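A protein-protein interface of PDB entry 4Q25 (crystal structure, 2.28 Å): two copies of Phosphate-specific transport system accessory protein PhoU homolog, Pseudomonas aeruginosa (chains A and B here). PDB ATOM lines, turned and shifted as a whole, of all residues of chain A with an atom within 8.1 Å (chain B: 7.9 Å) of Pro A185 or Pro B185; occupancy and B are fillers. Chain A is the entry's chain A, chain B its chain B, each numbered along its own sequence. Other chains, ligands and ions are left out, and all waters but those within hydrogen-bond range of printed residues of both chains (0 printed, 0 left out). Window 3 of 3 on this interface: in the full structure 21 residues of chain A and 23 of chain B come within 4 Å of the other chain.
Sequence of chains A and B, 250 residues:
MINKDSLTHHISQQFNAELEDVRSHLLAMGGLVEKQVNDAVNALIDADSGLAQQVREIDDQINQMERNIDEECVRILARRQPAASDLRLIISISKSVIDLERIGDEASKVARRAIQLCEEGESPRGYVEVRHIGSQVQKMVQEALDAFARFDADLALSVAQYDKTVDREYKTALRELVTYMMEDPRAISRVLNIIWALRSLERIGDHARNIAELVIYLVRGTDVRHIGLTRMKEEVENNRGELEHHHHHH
The guanidinium group (NH2) of Arg A190 sits at hydrogen-bond distance from the backbone carbonyl oxygen (O) of Arg A186 (3.4 Å).
Among the printed residues, pairs that only touch across the chains: Met A181 with Ile B188 (3.9 Å), Pro A185 with Met B182 (3.4 Å), Pro A185 with Pro B185 (3.8 Å), Arg A186 with Met B182 (3.9 Å), Ile A188 with Met B181 (3.8 Å), Ile A188 with Ile B188 (3.7 Å), Ser A189 with Val B178 (3.9 Å) and Ser A189 with Met B182 (3.7 Å).
Pro B185 touches just one residue of chain A: Pro A185 (3.8 Å).
Of the printed residues of chain B, Ile A188 touches Met B181 and Ile B188.
Of the printed residues of chain A, Ile B188 touches Met A181 and Ile A188.
Printed residues of chain A within 4 Å of Val B178: Ser A189 (3.9 Å).
Printed residues of chain B within 4 Å of Arg A186: Met B182 (3.9 Å).
Met A182 touches none of the printed residues of chain B.
Thr B179 touches none of the printed residues of chain A.
The nearest residue of chain B that does not touch Pro A185 is Ile B188 (4.5 Å).
The nearest residue of chain A that does not touch Pro B185 is Met A182 (5.1 Å).
Printed residues of chain B that touch a printed residue of chain A: Val B178, Met B181, Met B182, Pro B185 and Ile B188.
Of the 13 printed residues of chain A, 5 touch a printed residue of chain B.
Among the printed residues, 8 pairs touch across the chains.
Among the printed residues, no Asp or Glu carboxylate lies within 4 Å of a Lys or Arg side-chain nitrogen of the other chain.
Met A181 touches Ile B188, and with the chains exchanged Ile A188 touches Met B181.
Pro A185 touches Met B182, but with the chains exchanged Met A182 does not touch Pro B185 (5.1 Å).
Ile B188 touches its own counterpart, Ile A188.
Ser A189 touches Met B182, but with the chains exchanged Met A182 does not touch Ser B189 (5.3 Å).
Positions printed for both chains: 179, 180, 181, 182, 183, 184, 185, 186, 187, 188, 189 and 190.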
ATOM      1  N   THR A 179      25.153  -4.061 -26.798  1.00  0.00           N
ATOM      2  CA  THR A 179      24.094  -5.033 -27.110  1.00  0.00           C
ATOM      3  C   THR A 179      23.005  -4.938 -26.052  1.00  0.00           C
ATOM      4  O   THR A 179      21.811  -5.041 -26.359  1.00  0.00           O
ATOM      5  CB  THR A 179      24.622  -6.487 -27.254  1.00  0.00           C
ATOM      6  OG1 THR A 179      25.219  -6.907 -26.037  1.00  0.00           O
ATOM      7  CG2 THR A 179      25.709  -6.574 -28.342  1.00  0.00           C
ATOM      8  N   TYR A 180      23.398  -4.675 -24.804  1.00  0.00           N
ATOM      9  CA  TYR A 180      22.394  -4.469 -23.764  1.00  0.00           C
ATOM     10  C   TYR A 180      21.533  -3.217 -23.991  1.00  0.00           C
ATOM     11  O   TYR A 180      20.319  -3.265 -23.786  1.00  0.00           O
ATOM     12  CB  TYR A 180      22.991  -4.435 -22.369  1.00  0.00           C
ATOM     13  CG  TYR A 180      21.905  -4.280 -21.362  1.00  0.00           C
ATOM     14  CD1 TYR A 180      21.248  -5.384 -20.837  1.00  0.00           C
ATOM     15  CD2 TYR A 180      21.491  -3.025 -20.955  1.00  0.00           C
ATOM     16  CE1 TYR A 180      20.234  -5.243 -19.911  1.00  0.00           C
ATOM     17  CE2 TYR A 180      20.459  -2.886 -20.063  1.00  0.00           C
ATOM     18  CZ  TYR A 180      19.835  -3.995 -19.550  1.00  0.00           C
ATOM     19  OH  TYR A 180      18.816  -3.809 -18.652  1.00  0.00           O
ATOM     20  N   MET A 181      22.150  -2.110 -24.417  1.00  0.00           N
ATOM     21  CA  MET A 181      21.389  -0.885 -24.743  1.00  0.00           C
ATOM     22  C   MET A 181      20.308  -1.150 -25.787  1.00  0.00           C
ATOM     23  O   MET A 181      19.239  -0.548 -25.741  1.00  0.00           O
ATOM     24  CB  MET A 181      22.273   0.231 -25.287  1.00  0.00           C
ATOM     25  CG  MET A 181      23.047   0.933 -24.206  1.00  0.00           C
ATOM     26  SD  MET A 181      23.802   2.467 -24.742  1.00  0.00           S
ATOM     27  CE  MET A 181      25.086   1.832 -25.830  1.00  0.00           C
ATOM     28  N   MET A 182      20.593  -2.038 -26.725  1.00  0.00           N
ATOM     29  CA  MET A 182      19.667  -2.297 -27.821  1.00  0.00           C
ATOM     30  C   MET A 182      18.476  -3.112 -27.329  1.00  0.00           C
ATOM     31  O   MET A 182      17.384  -2.950 -27.809  1.00  0.00           O
ATOM     32  CB  MET A 182      20.400  -2.986 -28.952  1.00  0.00           C
ATOM     33  CG  MET A 182      21.579  -2.160 -29.452  1.00  0.00           C
ATOM     34  SD  MET A 182      22.325  -2.856 -30.918  1.00  0.00           S
ATOM     35  CE  MET A 182      20.910  -2.713 -32.024  1.00  0.00           C
ATOM     36  N   GLU A 183      18.703  -3.925 -26.310  1.00  0.00           N
ATOM     37  CA  GLU A 183      17.665  -4.695 -25.666  1.00  0.00           C
ATOM     38  C   GLU A 183      16.812  -3.837 -24.727  1.00  0.00           C
ATOM     39  O   GLU A 183      15.611  -4.070 -24.611  1.00  0.00           O
ATOM     40  CB  GLU A 183      18.302  -5.842 -24.887  1.00  0.00           C
ATOM     41  CG  GLU A 183      17.363  -6.637 -23.982  1.00  0.00           C
ATOM     42  CD  GLU A 183      18.090  -7.527 -22.971  1.00  0.00           C
ATOM     43  OE1 GLU A 183      19.337  -7.522 -22.952  1.00  0.00           O
ATOM     44  OE2 GLU A 183      17.420  -8.233 -22.175  1.00  0.00           O
ATOM     45  N   ASP A 184      17.422  -2.869 -24.043  1.00  0.00           N
ATOM     46  CA  ASP A 184      16.693  -2.031 -23.070  1.00  0.00           C
ATOM     47  C   ASP A 184      17.001  -0.559 -23.333  1.00  0.00           C
ATOM     48  O   ASP A 184      17.849   0.015 -22.664  1.00  0.00           O
ATOM     49  CB  ASP A 184      17.056  -2.429 -21.622  1.00  0.00           C
ATOM     50  CG  ASP A 184      16.357  -1.543 -20.537  1.00  0.00           C
ATOM     51  OD1 ASP A 184      15.361  -0.847 -20.809  1.00  0.00           O
ATOM     52  OD2 ASP A 184      16.819  -1.566 -19.371  1.00  0.00           O
ATOM     53  N   PRO A 185      16.330   0.039 -24.332  1.00  0.00           N
ATOM     54  CA  PRO A 185      16.593   1.407 -24.714  1.00  0.00           C
ATOM     55  C   PRO A 185      16.376   2.434 -23.602  1.00  0.00           C
ATOM     56  O   PRO A 185      17.045   3.460 -23.625  1.00  0.00           O
ATOM     57  CB  PRO A 185      15.619   1.641 -25.868  1.00  0.00           C
ATOM     58  CG  PRO A 185      15.446   0.330 -26.460  1.00  0.00           C
ATOM     59  CD  PRO A 185      15.452  -0.622 -25.307  1.00  0.00           C
ATOM     60  N   ARG A 186      15.487   2.169 -22.646  1.00  0.00           N
ATOM     61  CA  ARG A 186      15.284   3.079 -21.516  1.00  0.00           C
ATOM     62  C   ARG A 186      16.559   3.297 -20.682  1.00  0.00           C
ATOM     63  O   ARG A 186      16.665   4.241 -19.918  1.00  0.00           O
ATOM     64  CB  ARG A 186      14.176   2.560 -20.589  1.00  0.00           C
ATOM     65  CG  ARG A 186      12.775   2.431 -21.204  1.00  0.00           C
ATOM     66  CD  ARG A 186      11.728   2.272 -20.103  1.00  0.00           C
ATOM     67  NE  ARG A 186      10.437   1.769 -20.582  1.00  0.00           N
ATOM     68  CZ  ARG A 186      10.060   0.486 -20.594  1.00  0.00           C
ATOM     69  NH1 ARG A 186      10.872  -0.486 -20.157  1.00  0.00           N
ATOM     70  NH2 ARG A 186       8.850   0.170 -21.054  1.00  0.00           N
ATOM     71  N   ALA A 187      17.533   2.414 -20.819  1.00  0.00           N
ATOM     72  CA  ALA A 187      18.707   2.481 -19.984  1.00  0.00           C
ATOM     73  C   ALA A 187      19.900   3.148 -20.681  1.00  0.00           C
ATOM     74  O   ALA A 187      20.940   3.295 -20.078  1.00  0.00           O
ATOM     75  CB  ALA A 187      19.066   1.088 -19.505  1.00  0.00           C
ATOM     76  N   ILE A 188      19.716   3.606 -21.913  1.00  0.00           N
ATOM     77  CA  ILE A 188      20.786   4.155 -22.724  1.00  0.00           C
ATOM     78  C   ILE A 188      21.596   5.267 -22.050  1.00  0.00           C
ATOM     79  O   ILE A 188      22.831   5.258 -22.036  1.00  0.00           O
ATOM     80  CB  ILE A 188      20.218   4.656 -24.063  1.00  0.00           C
ATOM     81  CG1 ILE A 188      19.961   3.453 -24.992  1.00  0.00           C
ATOM     82  CG2 ILE A 188      21.152   5.679 -24.706  1.00  0.00           C
ATOM     83  CD1 ILE A 188      19.102   3.762 -26.201  1.00  0.00           C
ATOM     84  N   SER A 189      20.898   6.233 -21.482  1.00  0.00           N
ATOM     85  CA  SER A 189      21.535   7.336 -20.796  1.00  0.00           C
ATOM     86  C   SER A 189      22.405   6.853 -19.614  1.00  0.00           C
ATOM     87  O   SER A 189      23.524   7.351 -19.372  1.00  0.00           O
ATOM     88  CB  SER A 189      20.450   8.284 -20.325  1.00  0.00           C
ATOM     89  OG  SER A 189      20.998   9.396 -19.694  1.00  0.00           O
ATOM     90  N   ARG A 190      21.919   5.854 -18.892  1.00  0.00           N
ATOM     91  CA  ARG A 190      22.675   5.334 -17.776  1.00  0.00           C
ATOM     92  C   ARG A 190      23.850   4.455 -18.254  1.00  0.00           C
ATOM     93  O   ARG A 190      24.966   4.576 -17.742  1.00  0.00           O
ATOM     94  CB  ARG A 190      21.767   4.598 -16.809  1.00  0.00           C
ATOM     95  CG  ARG A 190      20.890   5.530 -16.001  1.00  0.00           C
ATOM     96  CD  ARG A 190      19.811   4.766 -15.250  1.00  0.00           C
ATOM     97  NE  ARG A 190      18.767   4.286 -16.154  1.00  0.00           N
ATOM     98  CZ  ARG A 190      18.131   3.122 -16.029  1.00  0.00           C
ATOM     99  NH1 ARG A 190      18.450   2.275 -15.071  1.00  0.00           N
ATOM    100  NH2 ARG A 190      17.194   2.791 -16.895  1.00  0.00           N
ATOM    101  N   VAL A 191      23.622   3.630 -19.264  1.00  0.00           N
ATOM    102  CA  VAL A 191      24.692   2.806 -19.814  1.00  0.00           C
ATOM    103  C   VAL A 191      25.810   3.630 -20.474  1.00  0.00           C
ATOM    104  O   VAL A 191      26.980   3.305 -20.339  1.00  0.00           O
ATOM    105  CB  VAL A 191      24.128   1.766 -20.800  1.00  0.00           C
ATOM    106  CG1 VAL A 191      25.236   1.017 -21.504  1.00  0.00           C
ATOM    107  CG2 VAL A 191      23.283   0.761 -20.047  1.00  0.00           C
ATOM    108  N   VAL B 178      20.421  11.252 -27.310  1.00  0.00           N
ATOM    109  CA  VAL B 178      19.994  10.175 -26.413  1.00  0.00           C
ATOM    110  C   VAL B 178      18.473   9.985 -26.350  1.00  0.00           C
ATOM    111  O   VAL B 178      17.941   8.879 -26.600  1.00  0.00           O
ATOM    112  CB  VAL B 178      20.524  10.411 -24.996  1.00  0.00           C
ATOM    113  CG1 VAL B 178      19.755   9.584 -23.989  1.00  0.00           C
ATOM    114  CG2 VAL B 178      22.002  10.057 -24.949  1.00  0.00           C
ATOM    115  N   THR B 179      17.763  11.071 -26.047  1.00  0.00           N
ATOM    116  CA  THR B 179      16.315  11.006 -25.989  1.00  0.00           C
ATOM    117  C   THR B 179      15.767  10.531 -27.340  1.00  0.00           C
ATOM    118  O   THR B 179      14.836   9.713 -27.394  1.00  0.00           O
ATOM    119  CB  THR B 179      15.679  12.332 -25.515  1.00  0.00           C
ATOM    120  OG1 THR B 179      15.915  13.357 -26.472  1.00  0.00           O
ATOM    121  CG2 THR B 179      16.261  12.791 -24.175  1.00  0.00           C
ATOM    122  N   TYR B 180      16.353  10.992 -28.436  1.00  0.00           N
ATOM    123  CA  TYR B 180      15.950  10.471 -29.733  1.00  0.00           C
ATOM    124  C   TYR B 180      16.155   8.947 -29.875  1.00  0.00           C
ATOM    125  O   TYR B 180      15.319   8.249 -30.466  1.00  0.00           O
ATOM    126  CB  TYR B 180      16.655  11.195 -30.887  1.00  0.00           C
ATOM    127  CG  TYR B 180      16.194  10.638 -32.222  1.00  0.00           C
ATOM    128  CD1 TYR B 180      14.983  11.034 -32.794  1.00  0.00           C
ATOM    129  CD2 TYR B 180      16.928   9.664 -32.868  1.00  0.00           C
ATOM    130  CE1 TYR B 180      14.546  10.478 -33.991  1.00  0.00           C
ATOM    131  CE2 TYR B 180      16.502   9.100 -34.047  1.00  0.00           C
ATOM    132  CZ  TYR B 180      15.312   9.507 -34.600  1.00  0.00           C
ATOM    133  OH  TYR B 180      14.916   8.943 -35.768  1.00  0.00           O
ATOM    134  N   MET B 181      17.267   8.418 -29.373  1.00  0.00           N
ATOM    135  CA  MET B 181      17.526   6.995 -29.503  1.00  0.00           C
ATOM    136  C   MET B 181      16.486   6.142 -28.744  1.00  0.00           C
ATOM    137  O   MET B 181      16.206   4.989 -29.108  1.00  0.00           O
ATOM    138  CB  MET B 181      18.926   6.669 -28.997  1.00  0.00           C
ATOM    139  CG  MET B 181      20.037   6.888 -30.005  1.00  0.00           C
ATOM    140  SD  MET B 181      21.574   6.299 -29.304  1.00  0.00           S
ATOM    141  CE  MET B 181      21.799   7.468 -27.975  1.00  0.00           C
ATOM    142  N   MET B 182      15.952   6.699 -27.666  1.00  0.00           N
ATOM    143  CA  MET B 182      14.867   6.060 -26.926  1.00  0.00           C
ATOM    144  C   MET B 182      13.524   6.172 -27.638  1.00  0.00           C
ATOM    145  O   MET B 182      12.688   5.295 -27.513  1.00  0.00           O
ATOM    146  CB  MET B 182      14.754   6.683 -25.566  1.00  0.00           C
ATOM    147  CG  MET B 182      15.980   6.485 -24.728  1.00  0.00           C
ATOM    148  SD  MET B 182      15.715   7.236 -23.118  1.00  0.00           S
ATOM    149  CE  MET B 182      17.392   7.112 -22.419  1.00  0.00           C
ATOM    150  N   GLU B 183      13.311   7.254 -28.377  1.00  0.00           N
ATOM    151  CA  GLU B 183      12.116   7.394 -29.202  1.00  0.00           C
ATOM    152  C   GLU B 183      12.201   6.461 -30.403  1.00  0.00           C
ATOM    153  O   GLU B 183      11.178   6.047 -30.936  1.00  0.00           O
ATOM    154  CB  GLU B 183      11.942   8.842 -29.678  1.00  0.00           C
ATOM    155  CG  GLU B 183      10.672   9.103 -30.496  1.00  0.00           C
ATOM    156  CD  GLU B 183      10.433  10.590 -30.812  1.00  0.00           C
ATOM    157  OE1 GLU B 183      10.803  11.042 -31.921  1.00  0.00           O
ATOM    158  OE2 GLU B 183       9.866  11.318 -29.960  1.00  0.00           O
ATOM    159  N   ASP B 184      13.415   6.125 -30.843  1.00  0.00           N
ATOM    160  CA  ASP B 184      13.577   5.283 -32.023  1.00  0.00           C
ATOM    161  C   ASP B 184      14.794   4.355 -31.920  1.00  0.00           C
ATOM    162  O   ASP B 184      15.854   4.620 -32.515  1.00  0.00           O
ATOM    163  CB  ASP B 184      13.624   6.151 -33.276  1.00  0.00           C
ATOM    164  CG  ASP B 184      13.887   5.344 -34.535  1.00  0.00           C
ATOM    165  OD1 ASP B 184      13.468   4.162 -34.620  1.00  0.00           O
ATOM    166  OD2 ASP B 184      14.534   5.900 -35.431  1.00  0.00           O
ATOM    167  N   PRO B 185      14.624   3.222 -31.212  1.00  0.00           N
ATOM    168  CA  PRO B 185      15.687   2.258 -30.894  1.00  0.00           C
ATOM    169  C   PRO B 185      16.401   1.658 -32.095  1.00  0.00           C
ATOM    170  O   PRO B 185      17.539   1.154 -31.977  1.00  0.00           O
ATOM    171  CB  PRO B 185      14.939   1.172 -30.129  1.00  0.00           C
ATOM    172  CG  PRO B 185      13.754   1.864 -29.553  1.00  0.00           C
ATOM    173  CD  PRO B 185      13.340   2.811 -30.620  1.00  0.00           C
ATOM    174  N   ARG B 186      15.750   1.695 -33.247  1.00  0.00           N
ATOM    175  CA  ARG B 186      16.340   1.120 -34.442  1.00  0.00           C
ATOM    176  C   ARG B 186      17.517   1.994 -34.940  1.00  0.00           C
ATOM    177  O   ARG B 186      18.370   1.530 -35.657  1.00  0.00           O
ATOM    178  CB  ARG B 186      15.271   0.916 -35.537  1.00  0.00           C
ATOM    179  CG  ARG B 186      14.833  -0.543 -35.713  1.00  0.00           C
ATOM    180  CD  ARG B 186      13.584  -0.685 -36.585  1.00  0.00           C
ATOM    181  NE  ARG B 186      12.349  -0.329 -35.866  1.00  0.00           N
ATOM    182  CZ  ARG B 186      11.517  -1.190 -35.258  1.00  0.00           C
ATOM    183  NH1 ARG B 186      11.744  -2.509 -35.259  1.00  0.00           N
ATOM    184  NH2 ARG B 186      10.434  -0.727 -34.637  1.00  0.00           N
ATOM    185  N   ALA B 187      17.566   3.250 -34.523  1.00  0.00           N
ATOM    186  CA  ALA B 187      18.616   4.151 -34.948  1.00  0.00           C
ATOM    187  C   ALA B 187      19.842   4.108 -34.025  1.00  0.00           C
ATOM    188  O   ALA B 187      20.796   4.844 -34.225  1.00  0.00           O
ATOM    189  CB  ALA B 187      18.062   5.557 -35.024  1.00  0.00           C
ATOM    190  N   ILE B 188      19.816   3.231 -33.033  1.00  0.00           N
ATOM    191  CA  ILE B 188      20.818   3.250 -31.968  1.00  0.00           C
ATOM    192  C   ILE B 188      22.235   3.206 -32.502  1.00  0.00           C
ATOM    193  O   ILE B 188      23.077   4.010 -32.111  1.00  0.00           O
ATOM    194  CB  ILE B 188      20.587   2.122 -30.953  1.00  0.00           C
ATOM    195  CG1 ILE B 188      19.458   2.548 -30.012  1.00  0.00           C
ATOM    196  CG2 ILE B 188      21.847   1.831 -30.134  1.00  0.00           C
ATOM    197  CD1 ILE B 188      18.948   1.456 -29.083  1.00  0.00           C
ATOM    198  N   SER B 189      22.477   2.289 -33.410  1.00  0.00           N
ATOM    199  CA  SER B 189      23.806   2.047 -33.935  1.00  0.00           C
ATOM    200  C   SER B 189      24.344   3.250 -34.752  1.00  0.00           C
ATOM    201  O   SER B 189      25.499   3.641 -34.644  1.00  0.00           O
ATOM    202  CB  SER B 189      23.775   0.783 -34.803  1.00  0.00           C
ATOM    203  OG  SER B 189      25.045   0.176 -34.829  1.00  0.00           O
ATOM    204  N   ARG B 190      23.486   3.832 -35.554  1.00  0.00           N
ATOM    205  CA  ARG B 190      23.838   4.987 -36.330  1.00  0.00           C
ATOM    206  C   ARG B 190      24.027   6.202 -35.406  1.00  0.00           C
ATOM    207  O   ARG B 190      25.012   6.932 -35.536  1.00  0.00           O
ATOM    208  CB  ARG B 190      22.772   5.250 -37.392  1.00  0.00           C
ATOM    209  CG  ARG B 190      22.819   4.248 -38.551  1.00  0.00           C
ATOM    210  CD  ARG B 190      21.630   4.391 -39.502  1.00  0.00           C
ATOM    211  NE  ARG B 190      20.421   3.878 -38.874  1.00  0.00           N
ATOM    212  CZ  ARG B 190      19.179   4.274 -39.120  1.00  0.00           C
ATOM    213  NH1 ARG B 190      18.919   5.210 -40.015  1.00  0.00           N
ATOM    214  NH2 ARG B 190      18.184   3.719 -38.447  1.00  0.00           N
